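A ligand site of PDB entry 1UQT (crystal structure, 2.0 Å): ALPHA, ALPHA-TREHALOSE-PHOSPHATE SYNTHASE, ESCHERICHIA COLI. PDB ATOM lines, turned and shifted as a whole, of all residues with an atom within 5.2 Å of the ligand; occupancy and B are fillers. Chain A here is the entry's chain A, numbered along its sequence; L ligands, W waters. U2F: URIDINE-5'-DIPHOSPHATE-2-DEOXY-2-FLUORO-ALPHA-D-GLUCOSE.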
ATOM      1  N   GLY A  23     -10.588  19.398  37.449  1.00  0.00           N
ATOM      2  CA  GLY A  23     -10.560  20.841  37.278  1.00  0.00           C
ATOM      3  C   GLY A  23     -11.503  21.615  38.162  1.00  0.00           C
ATOM      4  O   GLY A  23     -11.081  22.566  38.806  1.00  0.00           O
ATOM      5  N   TRP A  86     -29.223  18.150  28.744  1.00  0.00           N
ATOM      6  CA  TRP A  86     -27.888  18.126  28.136  1.00  0.00           C
ATOM      7  C   TRP A  86     -27.979  18.279  26.595  1.00  0.00           C
ATOM      8  O   TRP A  86     -27.314  19.123  26.043  1.00  0.00           O
ATOM      9  CB  TRP A  86     -27.070  16.883  28.505  1.00  0.00           C
ATOM     10  CG  TRP A  86     -25.772  16.848  27.829  1.00  0.00           C
ATOM     11  CD1 TRP A  86     -25.498  16.341  26.577  1.00  0.00           C
ATOM     12  CD2 TRP A  86     -24.515  17.328  28.345  1.00  0.00           C
ATOM     13  NE1 TRP A  86     -24.176  16.528  26.272  1.00  0.00           N
ATOM     14  CE2 TRP A  86     -23.540  17.088  27.355  1.00  0.00           C
ATOM     15  CE3 TRP A  86     -24.126  17.934  29.538  1.00  0.00           C
ATOM     16  CZ2 TRP A  86     -22.211  17.460  27.513  1.00  0.00           C
ATOM     17  CZ3 TRP A  86     -22.789  18.259  29.719  1.00  0.00           C
ATOM     18  CH2 TRP A  86     -21.855  18.054  28.699  1.00  0.00           C
ATOM     19  N   HIS A  90     -26.918  21.694  24.308  1.00  0.00           N
ATOM     20  CA  HIS A  90     -25.879  21.506  23.305  1.00  0.00           C
ATOM     21  C   HIS A  90     -26.446  21.502  21.878  1.00  0.00           C
ATOM     22  O   HIS A  90     -25.804  20.974  20.937  1.00  0.00           O
ATOM     23  CB  HIS A  90     -25.084  20.264  23.588  1.00  0.00           C
ATOM     24  CG  HIS A  90     -24.217  20.379  24.798  1.00  0.00           C
ATOM     25  ND1 HIS A  90     -24.706  20.235  26.080  1.00  0.00           N
ATOM     26  CD2 HIS A  90     -22.896  20.654  24.927  1.00  0.00           C
ATOM     27  CE1 HIS A  90     -23.721  20.417  26.948  1.00  0.00           C
ATOM     28  NE2 HIS A  90     -22.617  20.670  26.267  1.00  0.00           N
ATOM     29  N   PHE A 153     -23.776  28.491  39.040  1.00  0.00           N
ATOM     30  CA  PHE A 153     -22.888  28.496  37.898  1.00  0.00           C
ATOM     31  C   PHE A 153     -23.279  27.370  36.961  1.00  0.00           C
ATOM     32  O   PHE A 153     -23.380  26.217  37.369  1.00  0.00           O
ATOM     33  CB  PHE A 153     -21.426  28.398  38.298  1.00  0.00           C
ATOM     34  CG  PHE A 153     -20.486  28.535  37.124  1.00  0.00           C
ATOM     35  CD1 PHE A 153     -19.978  27.422  36.482  1.00  0.00           C
ATOM     36  CD2 PHE A 153     -20.199  29.789  36.606  1.00  0.00           C
ATOM     37  CE1 PHE A 153     -19.146  27.566  35.377  1.00  0.00           C
ATOM     38  CE2 PHE A 153     -19.407  29.933  35.486  1.00  0.00           C
ATOM     39  CZ  PHE A 153     -18.867  28.838  34.881  1.00  0.00           C
ATOM     40  N   HIS A 155     -22.140  25.211  33.851  1.00  0.00           N
ATOM     41  CA  HIS A 155     -20.879  24.773  33.304  1.00  0.00           C
ATOM     42  C   HIS A 155     -20.951  24.552  31.801  1.00  0.00           C
ATOM     43  O   HIS A 155     -19.920  24.394  31.171  1.00  0.00           O
ATOM     44  CB  HIS A 155     -20.402  23.513  33.983  1.00  0.00           C
ATOM     45  CG  HIS A 155     -19.924  23.752  35.368  1.00  0.00           C
ATOM     46  ND1 HIS A 155     -18.596  23.897  35.670  1.00  0.00           N
ATOM     47  CD2 HIS A 155     -20.615  23.910  36.534  1.00  0.00           C
ATOM     48  CE1 HIS A 155     -18.478  24.151  36.970  1.00  0.00           C
ATOM     49  NE2 HIS A 155     -19.681  24.141  37.517  1.00  0.00           N
ATOM     50  N   ILE A 156     -22.170  24.483  31.271  1.00  0.00           N
ATOM     51  CA  ILE A 156     -22.416  24.154  29.849  1.00  0.00           C
ATOM     52  C   ILE A 156     -23.048  25.370  29.183  1.00  0.00           C
ATOM     53  O   ILE A 156     -23.348  26.371  29.864  1.00  0.00           O
ATOM     54  CB  ILE A 156     -23.321  22.917  29.757  1.00  0.00           C
ATOM     55  CG1 ILE A 156     -24.743  23.201  30.246  1.00  0.00           C
ATOM     56  CG2 ILE A 156     -22.685  21.763  30.527  1.00  0.00           C
ATOM     57  CD1 ILE A 156     -25.736  22.054  30.097  1.00  0.00           C
ATOM     58  N   GLN A 186     -20.335  30.566  31.472  1.00  0.00           N
ATOM     59  CA  GLN A 186     -18.991  30.371  30.928  1.00  0.00           C
ATOM     60  C   GLN A 186     -18.563  31.476  29.982  1.00  0.00           C
ATOM     61  O   GLN A 186     -17.394  31.820  29.919  1.00  0.00           O
ATOM     62  CB  GLN A 186     -18.916  29.093  30.138  1.00  0.00           C
ATOM     63  CG  GLN A 186     -19.106  27.836  30.935  1.00  0.00           C
ATOM     64  CD  GLN A 186     -17.892  27.368  31.708  1.00  0.00           C
ATOM     65  OE1 GLN A 186     -16.952  28.141  32.009  1.00  0.00           O
ATOM     66  NE2 GLN A 186     -17.867  26.079  31.995  1.00  0.00           N
ATOM     67  N   ILE A 226     -14.318  29.201  33.300  1.00  0.00           N
ATOM     68  CA  ILE A 226     -13.550  28.344  34.221  1.00  0.00           C
ATOM     69  C   ILE A 226     -12.150  28.077  33.671  1.00  0.00           C
ATOM     70  O   ILE A 226     -11.919  27.999  32.449  1.00  0.00           O
ATOM     71  CB  ILE A 226     -14.308  27.037  34.484  1.00  0.00           C
ATOM     72  CG1 ILE A 226     -13.721  26.331  35.706  1.00  0.00           C
ATOM     73  CG2 ILE A 226     -14.316  26.142  33.270  1.00  0.00           C
ATOM     74  CD1 ILE A 226     -14.617  25.208  36.219  1.00  0.00           C
ATOM     75  N   VAL A 261      -8.466  14.113  24.053  1.00  0.00           N
ATOM     76  CA  VAL A 261      -9.073  13.445  25.166  1.00  0.00           C
ATOM     77  C   VAL A 261     -10.362  14.118  25.557  1.00  0.00           C
ATOM     78  O   VAL A 261     -10.440  15.334  25.680  1.00  0.00           O
ATOM     79  CB  VAL A 261      -8.082  13.313  26.348  1.00  0.00           C
ATOM     80  CG1 VAL A 261      -7.452  14.567  26.673  1.00  0.00           C
ATOM     81  CG2 VAL A 261      -8.785  12.724  27.575  1.00  0.00           C
ATOM     82  N   GLU A 262     -11.387  13.318  25.680  1.00  0.00           N
ATOM     83  CA  GLU A 262     -12.647  13.749  26.308  1.00  0.00           C
ATOM     84  C   GLU A 262     -13.526  12.576  26.641  1.00  0.00           C
ATOM     85  O   GLU A 262     -13.360  11.483  26.080  1.00  0.00           O
ATOM     86  CB  GLU A 262     -13.462  14.618  25.372  1.00  0.00           C
ATOM     87  CG  GLU A 262     -13.468  14.118  23.952  1.00  0.00           C
ATOM     88  CD  GLU A 262     -12.498  14.912  23.093  1.00  0.00           C
ATOM     89  OE1 GLU A 262     -12.829  16.067  22.691  1.00  0.00           O
ATOM     90  OE2 GLU A 262     -11.389  14.365  22.824  1.00  0.00           O
ATOM     91  N   ARG A 263     -14.498  12.822  27.499  1.00  0.00           N
ATOM     92  CA  ARG A 263     -15.666  11.964  27.583  1.00  0.00           C
ATOM     93  C   ARG A 263     -16.240  11.696  26.180  1.00  0.00           C
ATOM     94  O   ARG A 263     -16.307  12.605  25.349  1.00  0.00           O
ATOM     95  CB  ARG A 263     -16.767  12.566  28.446  1.00  0.00           C
ATOM     96  CG  ARG A 263     -16.463  12.713  29.935  1.00  0.00           C
ATOM     97  CD  ARG A 263     -17.621  13.396  30.713  1.00  0.00           C
ATOM     98  NE  ARG A 263     -17.989  14.664  30.091  1.00  0.00           N
ATOM     99  CZ  ARG A 263     -18.957  14.824  29.163  1.00  0.00           C
ATOM    100  NH1 ARG A 263     -19.745  13.824  28.811  1.00  0.00           N
ATOM    101  NH2 ARG A 263     -19.163  16.016  28.610  1.00  0.00           N
ATOM    102  N   LYS A 268     -18.831  16.495  21.621  1.00  0.00           N
ATOM    103  CA  LYS A 268     -17.400  16.639  21.374  1.00  0.00           C
ATOM    104  C   LYS A 268     -16.992  16.420  19.904  1.00  0.00           C
ATOM    105  O   LYS A 268     -15.836  16.593  19.574  1.00  0.00           O
ATOM    106  CB  LYS A 268     -16.613  15.663  22.246  1.00  0.00           C
ATOM    107  CG  LYS A 268     -16.881  15.777  23.736  1.00  0.00           C
ATOM    108  CD  LYS A 268     -16.295  17.045  24.345  1.00  0.00           C
ATOM    109  CE  LYS A 268     -16.742  17.178  25.815  1.00  0.00           C
ATOM    110  NZ  LYS A 268     -16.091  18.348  26.486  1.00  0.00           N
ATOM    111  N   ILE A 296      -8.423   9.442  23.273  1.00  0.00           N
ATOM    112  CA  ILE A 296      -8.830   8.867  24.552  1.00  0.00           C
ATOM    113  C   ILE A 296     -10.266   9.325  24.813  1.00  0.00           C
ATOM    114  O   ILE A 296     -10.580  10.504  24.735  1.00  0.00           O
ATOM    115  CB  ILE A 296      -7.869   9.283  25.673  1.00  0.00           C
ATOM    116  CG1 ILE A 296      -6.502   8.680  25.376  1.00  0.00           C
ATOM    117  CG2 ILE A 296      -8.419   8.837  27.017  1.00  0.00           C
ATOM    118  CD1 ILE A 296      -5.427   8.966  26.408  1.00  0.00           C
ATOM    119  N   PRO A 298     -13.137   7.903  27.328  1.00  0.00           N
ATOM    120  CA  PRO A 298     -13.860   7.059  28.293  1.00  0.00           C
ATOM    121  C   PRO A 298     -15.383   7.150  28.089  1.00  0.00           C
ATOM    122  O   PRO A 298     -15.890   8.222  27.853  1.00  0.00           O
ATOM    123  CB  PRO A 298     -13.504   7.687  29.669  1.00  0.00           C
ATOM    124  CG  PRO A 298     -13.080   9.048  29.361  1.00  0.00           C
ATOM    125  CD  PRO A 298     -12.395   8.971  28.004  1.00  0.00           C
ATOM    126  N   GLN A 338     -11.218   4.409  27.330  1.00  0.00           N
ATOM    127  CA  GLN A 338     -10.613   4.152  28.623  1.00  0.00           C
ATOM    128  C   GLN A 338     -10.382   5.453  29.365  1.00  0.00           C
ATOM    129  O   GLN A 338     -10.089   6.461  28.773  1.00  0.00           O
ATOM    130  CB  GLN A 338      -9.272   3.429  28.436  1.00  0.00           C
ATOM    131  CG  GLN A 338      -9.406   2.033  27.864  1.00  0.00           C
ATOM    132  CD  GLN A 338      -8.066   1.420  27.490  1.00  0.00           C
ATOM    133  OE1 GLN A 338      -7.083   1.541  28.245  1.00  0.00           O
ATOM    134  NE2 GLN A 338      -8.006   0.769  26.339  1.00  0.00           N
ATOM    135  N   HIS A 339     -10.489   5.426  30.678  1.00  0.00           N
ATOM    136  CA  HIS A 339     -10.236   6.609  31.463  1.00  0.00           C
ATOM    137  C   HIS A 339      -8.762   6.649  31.837  1.00  0.00           C
ATOM    138  O   HIS A 339      -8.194   5.646  32.236  1.00  0.00           O
ATOM    139  CB  HIS A 339     -11.130   6.617  32.699  1.00  0.00           C
ATOM    140  CG  HIS A 339     -10.750   7.633  33.727  1.00  0.00           C
ATOM    141  ND1 HIS A 339     -11.278   8.908  33.740  1.00  0.00           N
ATOM    142  CD2 HIS A 339      -9.957   7.545  34.829  1.00  0.00           C
ATOM    143  CE1 HIS A 339     -10.812   9.570  34.789  1.00  0.00           C
ATOM    144  NE2 HIS A 339     -10.000   8.766  35.460  1.00  0.00           N
ATOM    145  N   PHE A 340      -8.139   7.821  31.707  1.00  0.00           N
ATOM    146  CA  PHE A 340      -6.759   8.010  32.105  1.00  0.00           C
ATOM    147  C   PHE A 340      -6.705   8.993  33.249  1.00  0.00           C
ATOM    148  O   PHE A 340      -7.424   9.997  33.251  1.00  0.00           O
ATOM    149  CB  PHE A 340      -5.930   8.541  30.936  1.00  0.00           C
ATOM    150  CG  PHE A 340      -5.444   7.482  30.003  1.00  0.00           C
ATOM    151  CD1 PHE A 340      -6.344   6.743  29.242  1.00  0.00           C
ATOM    152  CD2 PHE A 340      -4.094   7.248  29.852  1.00  0.00           C
ATOM    153  CE1 PHE A 340      -5.909   5.770  28.390  1.00  0.00           C
ATOM    154  CE2 PHE A 340      -3.640   6.257  28.968  1.00  0.00           C
ATOM    155  CZ  PHE A 340      -4.544   5.511  28.246  1.00  0.00           C
ATOM    156  N   ASP A 341      -5.872   8.712  34.240  1.00  0.00           N
ATOM    157  CA  ASP A 341      -5.628   9.685  35.305  1.00  0.00           C
ATOM    158  C   ASP A 341      -5.190  11.051  34.754  1.00  0.00           C
ATOM    159  O   ASP A 341      -4.386  11.136  33.810  1.00  0.00           O
ATOM    160  CB  ASP A 341      -4.553   9.175  36.267  1.00  0.00           C
ATOM    161  CG  ASP A 341      -4.479  10.054  37.497  1.00  0.00           C
ATOM    162  OD1 ASP A 341      -3.555  10.896  37.573  1.00  0.00           O
ATOM    163  OD2 ASP A 341      -5.382  10.054  38.372  1.00  0.00           O
ATOM    164  N   ARG A 342      -5.730  12.096  35.350  1.00  0.00           N
ATOM    165  CA  ARG A 342      -5.474  13.475  34.910  1.00  0.00           C
ATOM    166  C   ARG A 342      -3.993  13.847  34.976  1.00  0.00           C
ATOM    167  O   ARG A 342      -3.457  14.531  34.103  1.00  0.00           O
ATOM    168  CB  ARG A 342      -6.292  14.438  35.772  1.00  0.00           C
ATOM    169  CG  ARG A 342      -6.410  15.835  35.195  1.00  0.00           C
ATOM    170  CD  ARG A 342      -7.456  16.676  35.903  1.00  0.00           C
ATOM    171  NE  ARG A 342      -7.375  18.037  35.418  1.00  0.00           N
ATOM    172  CZ  ARG A 342      -7.118  19.123  36.166  1.00  0.00           C
ATOM    173  NH1 ARG A 342      -6.939  19.048  37.487  1.00  0.00           N
ATOM    174  NH2 ARG A 342      -7.075  20.321  35.595  1.00  0.00           N
ATOM    175  N   LEU A 345      -2.247  12.363  32.095  1.00  0.00           N
ATOM    176  CA  LEU A 345      -2.620  13.067  30.881  1.00  0.00           C
ATOM    177  C   LEU A 345      -1.803  14.333  30.659  1.00  0.00           C
ATOM    178  O   LEU A 345      -1.490  14.677  29.532  1.00  0.00           O
ATOM    179  CB  LEU A 345      -4.104  13.414  30.861  1.00  0.00           C
ATOM    180  CG  LEU A 345      -5.130  12.335  30.566  1.00  0.00           C
ATOM    181  CD1 LEU A 345      -6.549  12.895  30.766  1.00  0.00           C
ATOM    182  CD2 LEU A 345      -4.996  11.732  29.156  1.00  0.00           C
ATOM    183  N   MET A 346      -1.441  15.044  31.724  1.00  0.00           N
ATOM    184  CA  MET A 346      -0.641  16.258  31.572  1.00  0.00           C
ATOM    185  C   MET A 346       0.695  15.902  30.957  1.00  0.00           C
ATOM    186  O   MET A 346       1.194  16.597  30.071  1.00  0.00           O
ATOM    187  CB  MET A 346      -0.413  16.948  32.922  1.00  0.00           C
ATOM    188  CG  MET A 346      -1.693  17.418  33.636  1.00  0.00           C
ATOM    189  SD  MET A 346      -2.848  18.340  32.614  1.00  0.00           S
ATOM    190  CE  MET A 346      -3.993  17.112  32.144  1.00  0.00           C
ATOM    191  N   ASP A 362     -19.315  23.318  23.391  1.00  0.00           N
ATOM    192  CA  ASP A 362     -18.722  23.060  24.703  1.00  0.00           C
ATOM    193  C   ASP A 362     -18.744  24.319  25.537  1.00  0.00           C
ATOM    194  O   ASP A 362     -18.339  25.375  25.060  1.00  0.00           O
ATOM    195  CB  ASP A 362     -17.293  22.564  24.536  1.00  0.00           C
ATOM    196  CG  ASP A 362     -16.967  21.334  25.364  1.00  0.00           C
ATOM    197  OD1 ASP A 362     -17.643  21.065  26.375  1.00  0.00           O
ATOM    198  OD2 ASP A 362     -16.028  20.557  25.063  1.00  0.00           O
ATOM    199  N   GLY A 363     -19.255  24.192  26.758  1.00  0.00           N
ATOM    200  CA  GLY A 363     -19.296  25.274  27.712  1.00  0.00           C
ATOM    201  C   GLY A 363     -17.948  25.983  27.779  1.00  0.00           C
ATOM    202  O   GLY A 363     -17.912  27.195  27.661  1.00  0.00           O
ATOM    203  N   MET A 364     -16.862  25.242  27.975  1.00  0.00           N
ATOM    204  CA  MET A 364     -15.533  25.841  27.989  1.00  0.00           C
ATOM    205  C   MET A 364     -14.548  24.915  27.298  1.00  0.00           C
ATOM    206  O   MET A 364     -14.035  25.209  26.220  1.00  0.00           O
ATOM    207  CB  MET A 364     -15.096  26.158  29.433  1.00  0.00           C
ATOM    208  CG  MET A 364     -13.753  26.866  29.561  1.00  0.00           C
ATOM    209  SD  MET A 364     -13.615  28.413  28.665  1.00  0.00           S
ATOM    210  CE  MET A 364     -15.118  29.216  29.132  1.00  0.00           C
ATOM    211  N   ASN A 365     -14.343  23.751  27.918  1.00  0.00           N
ATOM    212  CA  ASN A 365     -13.382  22.748  27.528  1.00  0.00           C
ATOM    213  C   ASN A 365     -12.061  23.026  28.212  1.00  0.00           C
ATOM    214  O   ASN A 365     -11.234  23.808  27.752  1.00  0.00           O
ATOM    215  CB  ASN A 365     -13.225  22.588  26.015  1.00  0.00           C
ATOM    216  CG  ASN A 365     -12.489  21.320  25.662  1.00  0.00           C
ATOM    217  OD1 ASN A 365     -11.328  21.128  26.098  1.00  0.00           O
ATOM    218  ND2 ASN A 365     -13.149  20.415  24.924  1.00  0.00           N
ATOM    219  N   LEU A 366     -11.906  22.379  29.356  1.00  0.00           N
ATOM    220  CA  LEU A 366     -10.713  22.485  30.136  1.00  0.00           C
ATOM    221  C   LEU A 366      -9.527  21.793  29.483  1.00  0.00           C
ATOM    222  O   LEU A 366      -8.408  22.210  29.672  1.00  0.00           O
ATOM    223  CB  LEU A 366     -10.948  21.882  31.493  1.00  0.00           C
ATOM    224  CG  LEU A 366     -11.800  22.780  32.349  1.00  0.00           C
ATOM    225  CD1 LEU A 366     -12.006  22.100  33.646  1.00  0.00           C
ATOM    226  CD2 LEU A 366     -11.114  24.100  32.550  1.00  0.00           C
ATOM    227  N   VAL A 367      -9.786  20.741  28.720  1.00  0.00           N
ATOM    228  CA  VAL A 367      -8.719  20.006  28.033  1.00  0.00           C
ATOM    229  C   VAL A 367      -7.892  20.951  27.183  1.00  0.00           C
ATOM    230  O   VAL A 367      -6.693  20.849  27.189  1.00  0.00           O
ATOM    231  CB  VAL A 367      -9.273  18.831  27.189  1.00  0.00           C
ATOM    232  CG1 VAL A 367      -8.242  18.316  26.168  1.00  0.00           C
ATOM    233  CG2 VAL A 367      -9.721  17.724  28.112  1.00  0.00           C
ATOM    234  N   GLU A 370      -5.704  22.836  29.657  1.00  0.00           N
ATOM    235  CA  GLU A 370      -4.722  21.894  30.172  1.00  0.00           C
ATOM    236  C   GLU A 370      -3.597  21.634  29.187  1.00  0.00           C
ATOM    237  O   GLU A 370      -2.423  21.612  29.542  1.00  0.00           O
ATOM    238  CB  GLU A 370      -5.361  20.555  30.527  1.00  0.00           C
ATOM    239  CG  GLU A 370      -6.252  20.633  31.775  1.00  0.00           C
ATOM    240  CD  GLU A 370      -7.181  19.441  31.944  1.00  0.00           C
ATOM    241  OE1 GLU A 370      -7.952  19.434  32.927  1.00  0.00           O
ATOM    242  OE2 GLU A 370      -7.196  18.533  31.106  1.00  0.00           O
HETATM  243  C1  U2F L   1     -18.187  19.929  31.478  1.00  0.00           C
HETATM  244  O1  U2F L   1     -17.016  18.856  31.534  1.00  0.00           O
HETATM  245  PB  U2F L   1     -16.283  18.187  30.283  1.00  0.00           P
HETATM  246  O1B U2F L   1     -16.204  16.700  30.521  1.00  0.00           O
HETATM  247  O2B U2F L   1     -17.456  18.247  29.331  1.00  0.00           O
HETATM  248  O3A U2F L   1     -15.026  18.609  29.447  1.00  0.00           O
HETATM  249  PA  U2F L   1     -13.704  19.273  30.015  1.00  0.00           P
HETATM  250  O1A U2F L   1     -14.010  20.587  30.494  1.00  0.00           O
HETATM  251  O2A U2F L   1     -12.715  19.219  28.865  1.00  0.00           O
HETATM  252  O5' U2F L   1     -13.257  18.417  31.294  1.00  0.00           O
HETATM  253  C5' U2F L   1     -12.774  17.115  31.045  1.00  0.00           C
HETATM  254  C4' U2F L   1     -11.903  16.830  32.276  1.00  0.00           C
HETATM  255  O4' U2F L   1     -11.738  15.430  32.459  1.00  0.00           O
HETATM  256  C1' U2F L   1     -10.342  15.130  32.435  1.00  0.00           C
HETATM  257  C2' U2F L   1      -9.721  16.154  31.551  1.00  0.00           C
HETATM  258  C3' U2F L   1     -10.501  17.357  32.010  1.00  0.00           C
HETATM  259  O3' U2F L   1      -9.950  17.894  33.181  1.00  0.00           O
HETATM  260  O2' U2F L   1      -8.362  16.274  31.792  1.00  0.00           O
HETATM  261  N1  U2F L   1     -10.288  13.778  31.927  1.00  0.00           N
HETATM  262  C6' U2F L   1      -9.479  12.868  32.609  1.00  0.00           C
HETATM  263  O6' U2F L   1      -8.943  13.178  33.635  1.00  0.00           O
HETATM  264  N3  U2F L   1      -9.438  11.541  32.195  1.00  0.00           N
HETATM  265  C7' U2F L   1     -10.109  11.140  31.084  1.00  0.00           C
HETATM  266  O7' U2F L   1     -10.008  10.085  30.757  1.00  0.00           O
HETATM  267  C8' U2F L   1     -10.858  12.069  30.351  1.00  0.00           C
HETATM  268  C9' U2F L   1     -10.963  13.393  30.787  1.00  0.00           C
HETATM  269  C2  U2F L   1     -18.502  20.929  30.437  1.00  0.00           C
HETATM  270  F1  U2F L   1     -19.051  20.277  29.317  1.00  0.00           F
HETATM  271  C3  U2F L   1     -17.203  21.691  29.830  1.00  0.00           C
HETATM  272  O3  U2F L   1     -17.275  22.496  28.489  1.00  0.00           O
HETATM  273  C4  U2F L   1     -16.598  22.602  30.952  1.00  0.00           C
HETATM  274  O4  U2F L   1     -15.175  23.006  30.503  1.00  0.00           O
HETATM  275  C5  U2F L   1     -16.545  21.698  32.386  1.00  0.00           C
HETATM  276  C6  U2F L   1     -16.191  22.709  33.564  1.00  0.00           C
HETATM  277  O6  U2F L   1     -16.894  23.942  33.597  1.00  0.00           O
HETATM  278  O5  U2F L   1     -17.836  21.053  32.512  1.00  0.00           O
HETATM  279  O   HOH W   1     -14.623  15.659  28.333  1.00  0.00           O
HETATM  280  O   HOH W   2     -20.488  21.701  27.630  1.00  0.00           O
HETATM  281  O   HOH W   3     -19.691  19.104  26.189  1.00  0.00           O
HETATM  282  O   HOH W   4     -13.258  17.453  26.976  1.00  0.00           O
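Water W2 lies within hydrogen-bond range of NE2 of His 90 (2.7 Å), N of Gly 363 (2.9 Å), OD1 of Asp 362 (3.2 Å) and O3 of the ligand (3.4 Å). Water W4 bridges O2A of the ligand (2.6 Å) and NZ of Lys 268 (3.0 Å). Water W1 bridges an oxygen (O1B) of the ligand (2.9 Å) and the backbone NH (N) of Arg 263 (3.0 Å). Water W3 bridges the side-chain carboxylate (OD1) of Asp 362 and a ring nitrogen (NE2) of His 90.
The backbone NH of Met 364 is in hydrogen-bond range of an oxygen (O3) of the ligand, 2.8 Å away. O1B of the ligand lies within salt-bridge range of NE of Arg 263, at 2.7 Å. An oxygen (O3) of the ligand lies within hydrogen-bond range of the side-chain carboxylate of Asp 362 (2.6 Å). The backbone NH (N) of Phe 340 lies within hydrogen-bond range of an oxygen (O7') of the ligand (3.1 Å). The side-chain amino group of Lys 268 lies within salt-bridge range of an oxygen (O2B) of the ligand (3.2 Å). The side-chain amide nitrogen (NE2) of Gln 186 is in hydrogen-bond range of an oxygen (O6) of the ligand, 2.8 Å away. The side-chain carboxylate of Glu 370 lies within hydrogen-bond range of an oxygen (O3') of the ligand, at 2.5 Å. ND1 of His 155 is in hydrogen-bond range of O6 of the ligand. N3 of the ligand lies within hydrogen-bond range of O of Phe 340 (2.7 Å). N of Asn 365 is in hydrogen-bond range of O4 of the ligand. The backbone NH of Val 367 lies within hydrogen-bond range of an oxygen (O2A) of the ligand. An oxygen (O3) of the ligand lies within hydrogen-bond range of the backbone NH (N) of Gly 363, 3.1 Å away. An oxygen (O3') of the ligand is in hydrogen-bond range of the guanidinium group of Arg 342 (3.4 Å). The backbone NH (N) of Leu 366 sits at hydrogen-bond distance from an oxygen (O1A) of the ligand, at 3.0 Å. A ring nitrogen (ND1) of His 339 sits at hydrogen-bond distance from an oxygen (O7') of the ligand (3.4 Å).
Merely in contact with the ligand: Ile 226 (3.4 Å), Leu 345 (3.5 Å), Val 261 (3.5 Å), Pro 298 (3.5 Å) and Trp 86 (3.6 Å). Of the 28 residues printed, 19 come within 4 Å of the ligand. The nearest printed residue that does not touch the ligand is Ile 156 (4.1 Å).
OD2 of Asp 362 lies within salt-bridge range of NZ of Lys 268, 2.6 Å away. O of Trp 86 sits at hydrogen-bond distance from ND1 of His 90 (2.8 Å). The backbone carbonyl oxygen (O) of His 155 lies within hydrogen-bond range of the side-chain amide nitrogen (NE2) of Gln 186 (2.8 Å). The side-chain amide nitrogen (ND2) of Asn 365 lies within hydrogen-bond range of the side-chain carboxylate (OD2) of Asp 362, at 2.9 Å. The backbone NH of Val 367 lies within hydrogen-bond range of the side-chain amide oxygen of Asn 365. The side-chain carboxylate of Glu 370 lies within salt-bridge range of the guanidinium group of Arg 342, at 2.9 Å. The backbone NH of Ile 226 sits at hydrogen-bond distance from the side-chain amide oxygen of Gln 186 (3.1 Å).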
